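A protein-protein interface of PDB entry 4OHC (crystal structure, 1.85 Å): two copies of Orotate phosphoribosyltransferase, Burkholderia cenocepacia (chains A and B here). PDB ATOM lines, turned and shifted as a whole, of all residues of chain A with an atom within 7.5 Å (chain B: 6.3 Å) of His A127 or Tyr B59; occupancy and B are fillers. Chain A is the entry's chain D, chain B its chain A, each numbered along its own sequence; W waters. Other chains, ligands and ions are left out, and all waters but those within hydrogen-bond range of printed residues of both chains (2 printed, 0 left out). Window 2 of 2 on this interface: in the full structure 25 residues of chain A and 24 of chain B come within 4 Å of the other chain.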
ATOM      1  N   ALA A  85      21.005   6.413 -14.030  1.00  0.00           N
ATOM      2  CA  ALA A  85      20.219   6.772 -15.194  1.00  0.00           C
ATOM      3  C   ALA A  85      20.592   8.187 -15.611  1.00  0.00           C
ATOM      4  O   ALA A  85      21.081   8.989 -14.794  1.00  0.00           O
ATOM      5  CB  ALA A  85      18.718   6.700 -14.857  1.00  0.00           C
ATOM      6  N   VAL A 106      23.530   2.965 -19.181  1.00  0.00           N
ATOM      7  CA  VAL A 106      22.484   3.120 -18.163  1.00  0.00           C
ATOM      8  C   VAL A 106      21.158   3.482 -18.837  1.00  0.00           C
ATOM      9  O   VAL A 106      21.155   4.016 -19.957  1.00  0.00           O
ATOM     10  CB  VAL A 106      22.784   4.160 -17.043  1.00  0.00           C
ATOM     11  CG1 VAL A 106      23.916   3.665 -16.123  1.00  0.00           C
ATOM     12  CG2 VAL A 106      23.097   5.531 -17.646  1.00  0.00           C
ATOM     13  N   PRO A 107      20.059   3.169 -18.179  1.00  0.00           N
ATOM     14  CA  PRO A 107      18.768   3.696 -18.637  1.00  0.00           C
ATOM     15  C   PRO A 107      18.784   5.215 -18.919  1.00  0.00           C
ATOM     16  O   PRO A 107      19.470   5.961 -18.257  1.00  0.00           O
ATOM     17  CB  PRO A 107      17.863   3.394 -17.450  1.00  0.00           C
ATOM     18  CG  PRO A 107      18.408   2.131 -16.894  1.00  0.00           C
ATOM     19  CD  PRO A 107      19.891   2.298 -16.990  1.00  0.00           C
ATOM     20  N   MET A 108      18.029   5.604 -19.941  1.00  0.00           N
ATOM     21  CA  MET A 108      17.763   6.987 -20.242  1.00  0.00           C
ATOM     22  C   MET A 108      16.270   7.295 -19.898  1.00  0.00           C
ATOM     23  O   MET A 108      15.439   6.437 -20.009  1.00  0.00           O
ATOM     24  CB  MET A 108      17.919   7.176 -21.744  1.00  0.00           C
ATOM     25  CG  MET A 108      17.557   8.542 -22.264  1.00  0.00           C
ATOM     26  SD  MET A 108      17.661   8.690 -24.037  1.00  0.00           S
ATOM     27  CE  MET A 108      17.150  10.467 -24.126  1.00  0.00           C
ATOM     28  N   GLN A 109      16.035   8.522 -19.463  1.00  0.00           N
ATOM     29  CA  GLN A 109      14.695   9.138 -19.453  1.00  0.00           C
ATOM     30  C   GLN A 109      14.803  10.487 -20.121  1.00  0.00           C
ATOM     31  O   GLN A 109      15.888  11.004 -20.402  1.00  0.00           O
ATOM     32  CB  GLN A 109      14.192   9.373 -18.032  1.00  0.00           C
ATOM     33  CG  GLN A 109      13.985   8.075 -17.264  1.00  0.00           C
ATOM     34  CD  GLN A 109      15.222   7.644 -16.545  1.00  0.00           C
ATOM     35  OE1 GLN A 109      16.030   8.476 -16.092  1.00  0.00           O
ATOM     36  NE2 GLN A 109      15.288   6.348 -16.252  1.00  0.00           N
ATOM     37  N   TYR A 110      13.636  11.102 -20.344  1.00  0.00           N
ATOM     38  CA  TYR A 110      13.657  12.538 -20.566  1.00  0.00           C
ATOM     39  C   TYR A 110      12.560  13.215 -19.760  1.00  0.00           C
ATOM     40  O   TYR A 110      11.620  12.582 -19.290  1.00  0.00           O
ATOM     41  CB  TYR A 110      13.640  12.910 -22.041  1.00  0.00           C
ATOM     42  CG  TYR A 110      12.440  12.564 -22.909  1.00  0.00           C
ATOM     43  CD1 TYR A 110      11.299  13.411 -22.968  1.00  0.00           C
ATOM     44  CD2 TYR A 110      12.466  11.461 -23.753  1.00  0.00           C
ATOM     45  CE1 TYR A 110      10.236  13.123 -23.834  1.00  0.00           C
ATOM     46  CE2 TYR A 110      11.390  11.162 -24.589  1.00  0.00           C
ATOM     47  CZ  TYR A 110      10.304  11.979 -24.654  1.00  0.00           C
ATOM     48  OH  TYR A 110       9.233  11.680 -25.537  1.00  0.00           O
ATOM     49  N   ASN A 121       4.942  10.470 -12.123  1.00  0.00           N
ATOM     50  CA  ASN A 121       5.717  10.384 -13.339  1.00  0.00           C
ATOM     51  C   ASN A 121       5.209  11.266 -14.513  1.00  0.00           C
ATOM     52  O   ASN A 121       5.704  11.140 -15.665  1.00  0.00           O
ATOM     53  CB  ASN A 121       5.773   8.917 -13.755  1.00  0.00           C
ATOM     54  CG  ASN A 121       6.459   8.050 -12.712  1.00  0.00           C
ATOM     55  OD1 ASN A 121       5.804   7.421 -11.892  1.00  0.00           O
ATOM     56  ND2 ASN A 121       7.783   8.027 -12.735  1.00  0.00           N
ATOM     57  N   ILE A 124       7.804  12.876 -16.653  1.00  0.00           N
ATOM     58  CA  ILE A 124       8.907  11.981 -17.094  1.00  0.00           C
ATOM     59  C   ILE A 124       8.446  11.110 -18.239  1.00  0.00           C
ATOM     60  O   ILE A 124       7.315  10.635 -18.222  1.00  0.00           O
ATOM     61  CB  ILE A 124       9.334  10.989 -15.953  1.00  0.00           C
ATOM     62  CG1 ILE A 124       9.634  11.764 -14.690  1.00  0.00           C
ATOM     63  CG2 ILE A 124      10.534  10.113 -16.360  1.00  0.00           C
ATOM     64  CD1 ILE A 124      10.606  12.906 -14.950  1.00  0.00           C
ATOM     65  N   GLU A 125       9.297  10.922 -19.245  1.00  0.00           N
ATOM     66  CA  GLU A 125       9.091   9.905 -20.235  1.00  0.00           C
ATOM     67  C   GLU A 125      10.225   8.894 -20.156  1.00  0.00           C
ATOM     68  O   GLU A 125      11.405   9.237 -19.948  1.00  0.00           O
ATOM     69  CB  GLU A 125       8.938  10.484 -21.640  1.00  0.00           C
ATOM     70  CG  GLU A 125       7.745  11.475 -21.799  1.00  0.00           C
ATOM     71  CD  GLU A 125       6.375  10.882 -21.552  1.00  0.00           C
ATOM     72  OE1 GLU A 125       6.224   9.654 -21.765  1.00  0.00           O
ATOM     73  OE2 GLU A 125       5.434  11.635 -21.150  1.00  0.00           O
ATOM     74  N   GLY A 126       9.852   7.644 -20.309  1.00  0.00           N
ATOM     75  CA  GLY A 126      10.732   6.538 -20.097  1.00  0.00           C
ATOM     76  C   GLY A 126      10.331   5.873 -18.802  1.00  0.00           C
ATOM     77  O   GLY A 126       9.313   6.262 -18.169  1.00  0.00           O
ATOM     78  N   HIS A 127      11.098   4.875 -18.413  1.00  0.00           N
ATOM     79  CA  HIS A 127      10.848   4.150 -17.186  1.00  0.00           C
ATOM     80  C   HIS A 127      11.890   4.539 -16.157  1.00  0.00           C
ATOM     81  O   HIS A 127      13.065   4.477 -16.437  1.00  0.00           O
ATOM     82  CB  HIS A 127      10.929   2.659 -17.456  1.00  0.00           C
ATOM     83  CG  HIS A 127      10.763   1.858 -16.226  1.00  0.00           C
ATOM     84  ND1 HIS A 127      11.822   1.229 -15.608  1.00  0.00           N
ATOM     85  CD2 HIS A 127       9.690   1.670 -15.435  1.00  0.00           C
ATOM     86  CE1 HIS A 127      11.381   0.618 -14.523  1.00  0.00           C
ATOM     87  NE2 HIS A 127      10.101   0.890 -14.382  1.00  0.00           N
ATOM     88  N   LEU A 128      11.463   4.971 -14.997  1.00  0.00           N
ATOM     89  CA  LEU A 128      12.356   5.433 -13.957  1.00  0.00           C
ATOM     90  C   LEU A 128      12.144   4.619 -12.695  1.00  0.00           C
ATOM     91  O   LEU A 128      11.116   4.722 -12.079  1.00  0.00           O
ATOM     92  CB  LEU A 128      12.058   6.876 -13.628  1.00  0.00           C
ATOM     93  CG  LEU A 128      12.963   7.424 -12.496  1.00  0.00           C
ATOM     94  CD1 LEU A 128      14.435   7.402 -12.825  1.00  0.00           C
ATOM     95  CD2 LEU A 128      12.544   8.839 -12.172  1.00  0.00           C
ATOM     96  N   GLU A 129      13.125   3.813 -12.321  1.00  0.00           N
ATOM     97  CA  GLU A 129      13.041   3.013 -11.074  1.00  0.00           C
ATOM     98  C   GLU A 129      13.170   3.891  -9.844  1.00  0.00           C
ATOM     99  O   GLU A 129      14.129   4.647  -9.738  1.00  0.00           O
ATOM    100  CB  GLU A 129      14.150   1.965 -11.087  1.00  0.00           C
ATOM    101  N   GLU A 130      12.220   3.777  -8.895  1.00  0.00           N
ATOM    102  CA  GLU A 130      12.262   4.497  -7.603  1.00  0.00           C
ATOM    103  C   GLU A 130      13.661   4.282  -6.978  1.00  0.00           C
ATOM    104  O   GLU A 130      14.239   3.165  -7.050  1.00  0.00           O
ATOM    105  CB  GLU A 130      11.115   4.020  -6.623  1.00  0.00           C
ATOM    106  N   SER A 132      16.521   5.538  -8.084  1.00  0.00           N
ATOM    107  CA  SER A 132      17.595   5.775  -9.051  1.00  0.00           C
ATOM    108  C   SER A 132      18.306   7.125  -8.848  1.00  0.00           C
ATOM    109  O   SER A 132      17.652   8.147  -8.640  1.00  0.00           O
ATOM    110  CB  SER A 132      17.042   5.805 -10.466  1.00  0.00           C
ATOM    111  OG  SER A 132      16.478   4.567 -10.847  1.00  0.00           O
ATOM    112  N   VAL B  28       9.197  -5.884 -21.915  1.00  0.00           N
ATOM    113  CA  VAL B  28       9.310  -4.758 -21.010  1.00  0.00           C
ATOM    114  C   VAL B  28       7.997  -3.992 -20.816  1.00  0.00           C
ATOM    115  O   VAL B  28       8.025  -2.935 -20.240  1.00  0.00           O
ATOM    116  CB  VAL B  28      10.421  -3.794 -21.358  1.00  0.00           C
ATOM    117  CG1 VAL B  28      11.754  -4.552 -21.432  1.00  0.00           C
ATOM    118  CG2 VAL B  28      10.127  -3.045 -22.673  1.00  0.00           C
ATOM    119  N   ARG B  54       8.324   5.203 -25.843  1.00  0.00           N
ATOM    120  CA  ARG B  54       9.320   5.981 -25.050  1.00  0.00           C
ATOM    121  C   ARG B  54       9.946   5.129 -23.937  1.00  0.00           C
ATOM    122  O   ARG B  54      11.127   5.352 -23.523  1.00  0.00           O
ATOM    123  CB  ARG B  54       8.683   7.264 -24.477  1.00  0.00           C
ATOM    124  CG  ARG B  54       8.262   8.174 -25.615  1.00  0.00           C
ATOM    125  CD  ARG B  54       7.195   9.210 -25.278  1.00  0.00           C
ATOM    126  NE  ARG B  54       6.085   8.617 -24.557  1.00  0.00           N
ATOM    127  CZ  ARG B  54       4.921   9.217 -24.367  1.00  0.00           C
ATOM    128  NH1 ARG B  54       4.716  10.458 -24.869  1.00  0.00           N
ATOM    129  NH2 ARG B  54       3.972   8.613 -23.644  1.00  0.00           N
ATOM    130  N   LYS B  55       9.211   4.123 -23.474  1.00  0.00           N
ATOM    131  CA  LYS B  55       9.691   3.249 -22.407  1.00  0.00           C
ATOM    132  C   LYS B  55      11.004   2.575 -22.827  1.00  0.00           C
ATOM    133  O   LYS B  55      11.871   2.271 -21.980  1.00  0.00           O
ATOM    134  CB  LYS B  55       8.639   2.204 -22.103  1.00  0.00           C
ATOM    135  CG  LYS B  55       8.734   1.572 -20.748  1.00  0.00           C
ATOM    136  CD  LYS B  55       7.629   0.536 -20.610  1.00  0.00           C
ATOM    137  CE  LYS B  55       7.526   0.035 -19.193  1.00  0.00           C
ATOM    138  NZ  LYS B  55       8.860  -0.409 -18.841  1.00  0.00           N
ATOM    139  N   LEU B  56      11.141   2.360 -24.116  1.00  0.00           N
ATOM    140  CA  LEU B  56      12.234   1.542 -24.669  1.00  0.00           C
ATOM    141  C   LEU B  56      13.620   2.177 -24.455  1.00  0.00           C
ATOM    142  O   LEU B  56      14.638   1.489 -24.395  1.00  0.00           O
ATOM    143  CB  LEU B  56      11.957   1.257 -26.137  1.00  0.00           C
ATOM    144  CG  LEU B  56      10.651   0.489 -26.391  1.00  0.00           C
ATOM    145  CD1 LEU B  56      10.284   0.537 -27.851  1.00  0.00           C
ATOM    146  CD2 LEU B  56      10.642  -0.975 -25.845  1.00  0.00           C
ATOM    147  N   ILE B  57      13.664   3.483 -24.315  1.00  0.00           N
ATOM    148  CA  ILE B  57      14.916   4.188 -24.083  1.00  0.00           C
ATOM    149  C   ILE B  57      15.572   3.889 -22.720  1.00  0.00           C
ATOM    150  O   ILE B  57      16.736   4.189 -22.519  1.00  0.00           O
ATOM    151  CB  ILE B  57      14.772   5.722 -24.253  1.00  0.00           C
ATOM    152  CG1 ILE B  57      14.091   6.345 -23.040  1.00  0.00           C
ATOM    153  CG2 ILE B  57      14.069   6.044 -25.591  1.00  0.00           C
ATOM    154  CD1 ILE B  57      13.719   7.824 -23.242  1.00  0.00           C
ATOM    155  N   SER B  58      14.793   3.342 -21.811  1.00  0.00           N
ATOM    156  CA  SER B  58      15.190   3.054 -20.454  1.00  0.00           C
ATOM    157  C   SER B  58      15.768   1.638 -20.233  1.00  0.00           C
ATOM    158  O   SER B  58      16.091   1.298 -19.109  1.00  0.00           O
ATOM    159  CB  SER B  58      13.991   3.288 -19.525  1.00  0.00           C
ATOM    160  OG  SER B  58      13.385   4.572 -19.767  1.00  0.00           O
ATOM    161  N   TYR B  59      15.993   0.870 -21.294  1.00  0.00           N
ATOM    162  CA  TYR B  59      16.467  -0.503 -21.193  1.00  0.00           C
ATOM    163  C   TYR B  59      17.685  -0.700 -22.138  1.00  0.00           C
ATOM    164  O   TYR B  59      17.506  -0.864 -23.317  1.00  0.00           O
ATOM    165  CB  TYR B  59      15.310  -1.451 -21.596  1.00  0.00           C
ATOM    166  CG  TYR B  59      14.154  -1.416 -20.637  1.00  0.00           C
ATOM    167  CD1 TYR B  59      14.226  -2.087 -19.451  1.00  0.00           C
ATOM    168  CD2 TYR B  59      13.033  -0.628 -20.889  1.00  0.00           C
ATOM    169  CE1 TYR B  59      13.198  -2.016 -18.527  1.00  0.00           C
ATOM    170  CE2 TYR B  59      12.027  -0.510 -19.989  1.00  0.00           C
ATOM    171  CZ  TYR B  59      12.057  -1.264 -18.832  1.00  0.00           C
ATOM    172  OH  TYR B  59      11.028  -1.147 -17.885  1.00  0.00           O
ATOM    173  N   PRO B  60      18.922  -0.653 -21.598  1.00  0.00           N
ATOM    174  CA  PRO B  60      20.089  -0.637 -22.446  1.00  0.00           C
ATOM    175  C   PRO B  60      20.215  -1.788 -23.464  1.00  0.00           C
ATOM    176  O   PRO B  60      20.646  -1.520 -24.617  1.00  0.00           O
ATOM    177  CB  PRO B  60      21.239  -0.677 -21.452  1.00  0.00           C
ATOM    178  CG  PRO B  60      20.703  -0.019 -20.244  1.00  0.00           C
ATOM    179  CD  PRO B  60      19.279  -0.447 -20.187  1.00  0.00           C
ATOM    180  N   ARG B  61      19.918  -3.019 -23.079  1.00  0.00           N
ATOM    181  CA  ARG B  61      20.071  -4.151 -24.025  1.00  0.00           C
ATOM    182  C   ARG B  61      18.943  -4.136 -25.109  1.00  0.00           C
ATOM    183  O   ARG B  61      19.164  -4.381 -26.326  1.00  0.00           O
ATOM    184  CB  ARG B  61      20.112  -5.494 -23.286  1.00  0.00           C
ATOM    185  CG  ARG B  61      21.402  -5.680 -22.474  1.00  0.00           C
ATOM    186  CD  ARG B  61      21.172  -6.535 -21.244  1.00  0.00           C
ATOM    187  NE  ARG B  61      20.420  -5.661 -20.353  1.00  0.00           N
ATOM    188  CZ  ARG B  61      20.949  -4.649 -19.649  1.00  0.00           C
ATOM    189  NH1 ARG B  61      22.239  -4.453 -19.566  1.00  0.00           N
ATOM    190  NH2 ARG B  61      20.169  -3.801 -18.988  1.00  0.00           N
ATOM    191  N   VAL B  62      17.744  -3.831 -24.635  1.00  0.00           N
ATOM    192  CA  VAL B  62      16.606  -3.629 -25.527  1.00  0.00           C
ATOM    193  C   VAL B  62      16.845  -2.530 -26.563  1.00  0.00           C
ATOM    194  O   VAL B  62      16.639  -2.728 -27.762  1.00  0.00           O
ATOM    195  CB  VAL B  62      15.308  -3.334 -24.732  1.00  0.00           C
ATOM    196  CG1 VAL B  62      14.301  -2.512 -25.524  1.00  0.00           C
ATOM    197  CG2 VAL B  62      14.674  -4.633 -24.324  1.00  0.00           C
ATOM    198  N   ARG B  63      17.323  -1.381 -26.133  1.00  0.00           N
ATOM    199  CA  ARG B  63      17.451  -0.294 -27.101  1.00  0.00           C
ATOM    200  C   ARG B  63      18.551  -0.586 -28.093  1.00  0.00           C
ATOM    201  O   ARG B  63      18.438  -0.250 -29.282  1.00  0.00           O
ATOM    202  CB  ARG B  63      17.591   1.088 -26.425  1.00  0.00           C
ATOM    203  CG  ARG B  63      18.976   1.349 -25.854  1.00  0.00           C
ATOM    204  CD  ARG B  63      18.973   2.539 -24.863  1.00  0.00           C
ATOM    205  NE  ARG B  63      20.304   2.638 -24.272  1.00  0.00           N
ATOM    206  CZ  ARG B  63      20.561   3.160 -23.079  1.00  0.00           C
ATOM    207  NH1 ARG B  63      19.589   3.703 -22.341  1.00  0.00           N
ATOM    208  NH2 ARG B  63      21.797   3.154 -22.616  1.00  0.00           N
ATOM    209  N   ARG B  64      19.611  -1.192 -27.631  1.00  0.00           N
ATOM    210  CA  ARG B  64      20.668  -1.634 -28.541  1.00  0.00           C
ATOM    211  C   ARG B  64      20.109  -2.551 -29.666  1.00  0.00           C
ATOM    212  O   ARG B  64      20.430  -2.366 -30.854  1.00  0.00           O
ATOM    213  CB  ARG B  64      21.749  -2.320 -27.739  1.00  0.00           C
ATOM    214  CG  ARG B  64      22.850  -2.868 -28.587  1.00  0.00           C
ATOM    215  CD  ARG B  64      24.088  -3.272 -27.786  1.00  0.00           C
ATOM    216  NE  ARG B  64      23.863  -4.427 -26.924  1.00  0.00           N
ATOM    217  CZ  ARG B  64      24.707  -4.895 -26.009  1.00  0.00           C
ATOM    218  NH1 ARG B  64      25.873  -4.277 -25.755  1.00  0.00           N
ATOM    219  NH2 ARG B  64      24.367  -5.960 -25.325  1.00  0.00           N
HETATM  220  O   HOH W   1       2.672  10.701 -21.727  1.00  0.00           O
HETATM  221  O   HOH W   2      14.882   1.287 -16.545  1.00  0.00           O
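Water W2 bridges O of Ser B58 (2.8 Å) and ND1 of His A127 (3.2 Å). Water W1 bridges OE2 of Glu A125 (3.0 Å) and NH2 of Arg B54 (3.1 Å).
The side-chain amino group of Lys B55 sits at hydrogen-bond distance from the backbone carbonyl oxygen of Val B28, at 3.0 Å. The side-chain hydroxyl of Tyr B59 sits at hydrogen-bond distance from the side-chain amino group of Lys B55. The backbone carbonyl oxygen (O) of Ile B57 sits at hydrogen-bond distance from the guanidinium group (NH1) of Arg B63. The side-chain amide nitrogen of Gln A109 lies within hydrogen-bond range of the backbone carbonyl oxygen of His A127, at 2.9 Å. O of Tyr A110 is in hydrogen-bond range of N of Glu A125, at 2.9 Å.
Among the printed residues, merely in contact across the chains: Pro A107 with Ser B58 (3.2 Å), Tyr A110 with Arg B54 (3.2 Å), Gly A126 with Ser B58 (3.3 Å), Gly A126 with Arg B54 (3.6 Å), Pro A107 with Arg B63 (3.8 Å), Val A106 with Pro B60 (3.8 Å), Pro A107 with Pro B60 (3.9 Å), Tyr A110 with Ile B57 (3.9 Å) and His A127 with Lys B55 (3.9 Å).
Of the printed residues of chain B, Pro A107 touches Ser B58, Pro B60 and Arg B63. Asn A121 touches none of the printed residues of chain B. Printed residues of chain B within 4 Å of His A127: Lys B55, Ser B58 and Tyr B59. Leu A128 touches none of the printed residues of chain B. Tyr B59 touches just one residue of chain A: His A127 (3.4 Å). Of the printed residues of chain A, Arg B63 touches Val A106 (2.9 Å), Pro A107 (3.8 Å) and Met A108 (3.4 Å). The nearest residue of chain A that does not touch Tyr B59 is Pro A107 (4.8 Å). The nearest printed residue of chain B that does not touch Glu A125 is Ile B57 (4.3 Å).
The guanidinium group (NE) of Arg B54 is in salt-bridge range of the side-chain carboxylate (OE1) of Glu A125. The backbone carbonyl oxygen of Ile B57 sits at hydrogen-bond distance from the backbone NH of Met A108 (3.2 Å). The backbone carbonyl oxygen of Met A108 sits at hydrogen-bond distance from the side-chain hydroxyl of Ser B58, 2.8 Å away. The backbone NH (N) of His A127 lies within hydrogen-bond range of the side-chain hydroxyl (OG) of Ser B58, at 2.7 Å. ND1 of His A127 lies within hydrogen-bond range of OH of Tyr B59 (3.4 Å). O of Val A106 is in hydrogen-bond range of NH2 of Arg B63. N of Met A108 lies close to NH1 of Arg B63 (3.4 Å).
Along chain B the printed residues that touch a printed residue of chain A span positions 54 to 63. Hydrophobic or aromatic side chains of chain A within 4 Å of the printed part of chain B: Pro A107, Met A108, Tyr A110 and His A127. Among the printed residues, 16 pairs touch across the chains. Among the printed residues, Asp or Glu carboxylates within 4 Å of a Lys or Arg side-chain nitrogen of the other chain: Glu A125 with Arg B54 (3.0 Å).
No position is printed for both chains.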
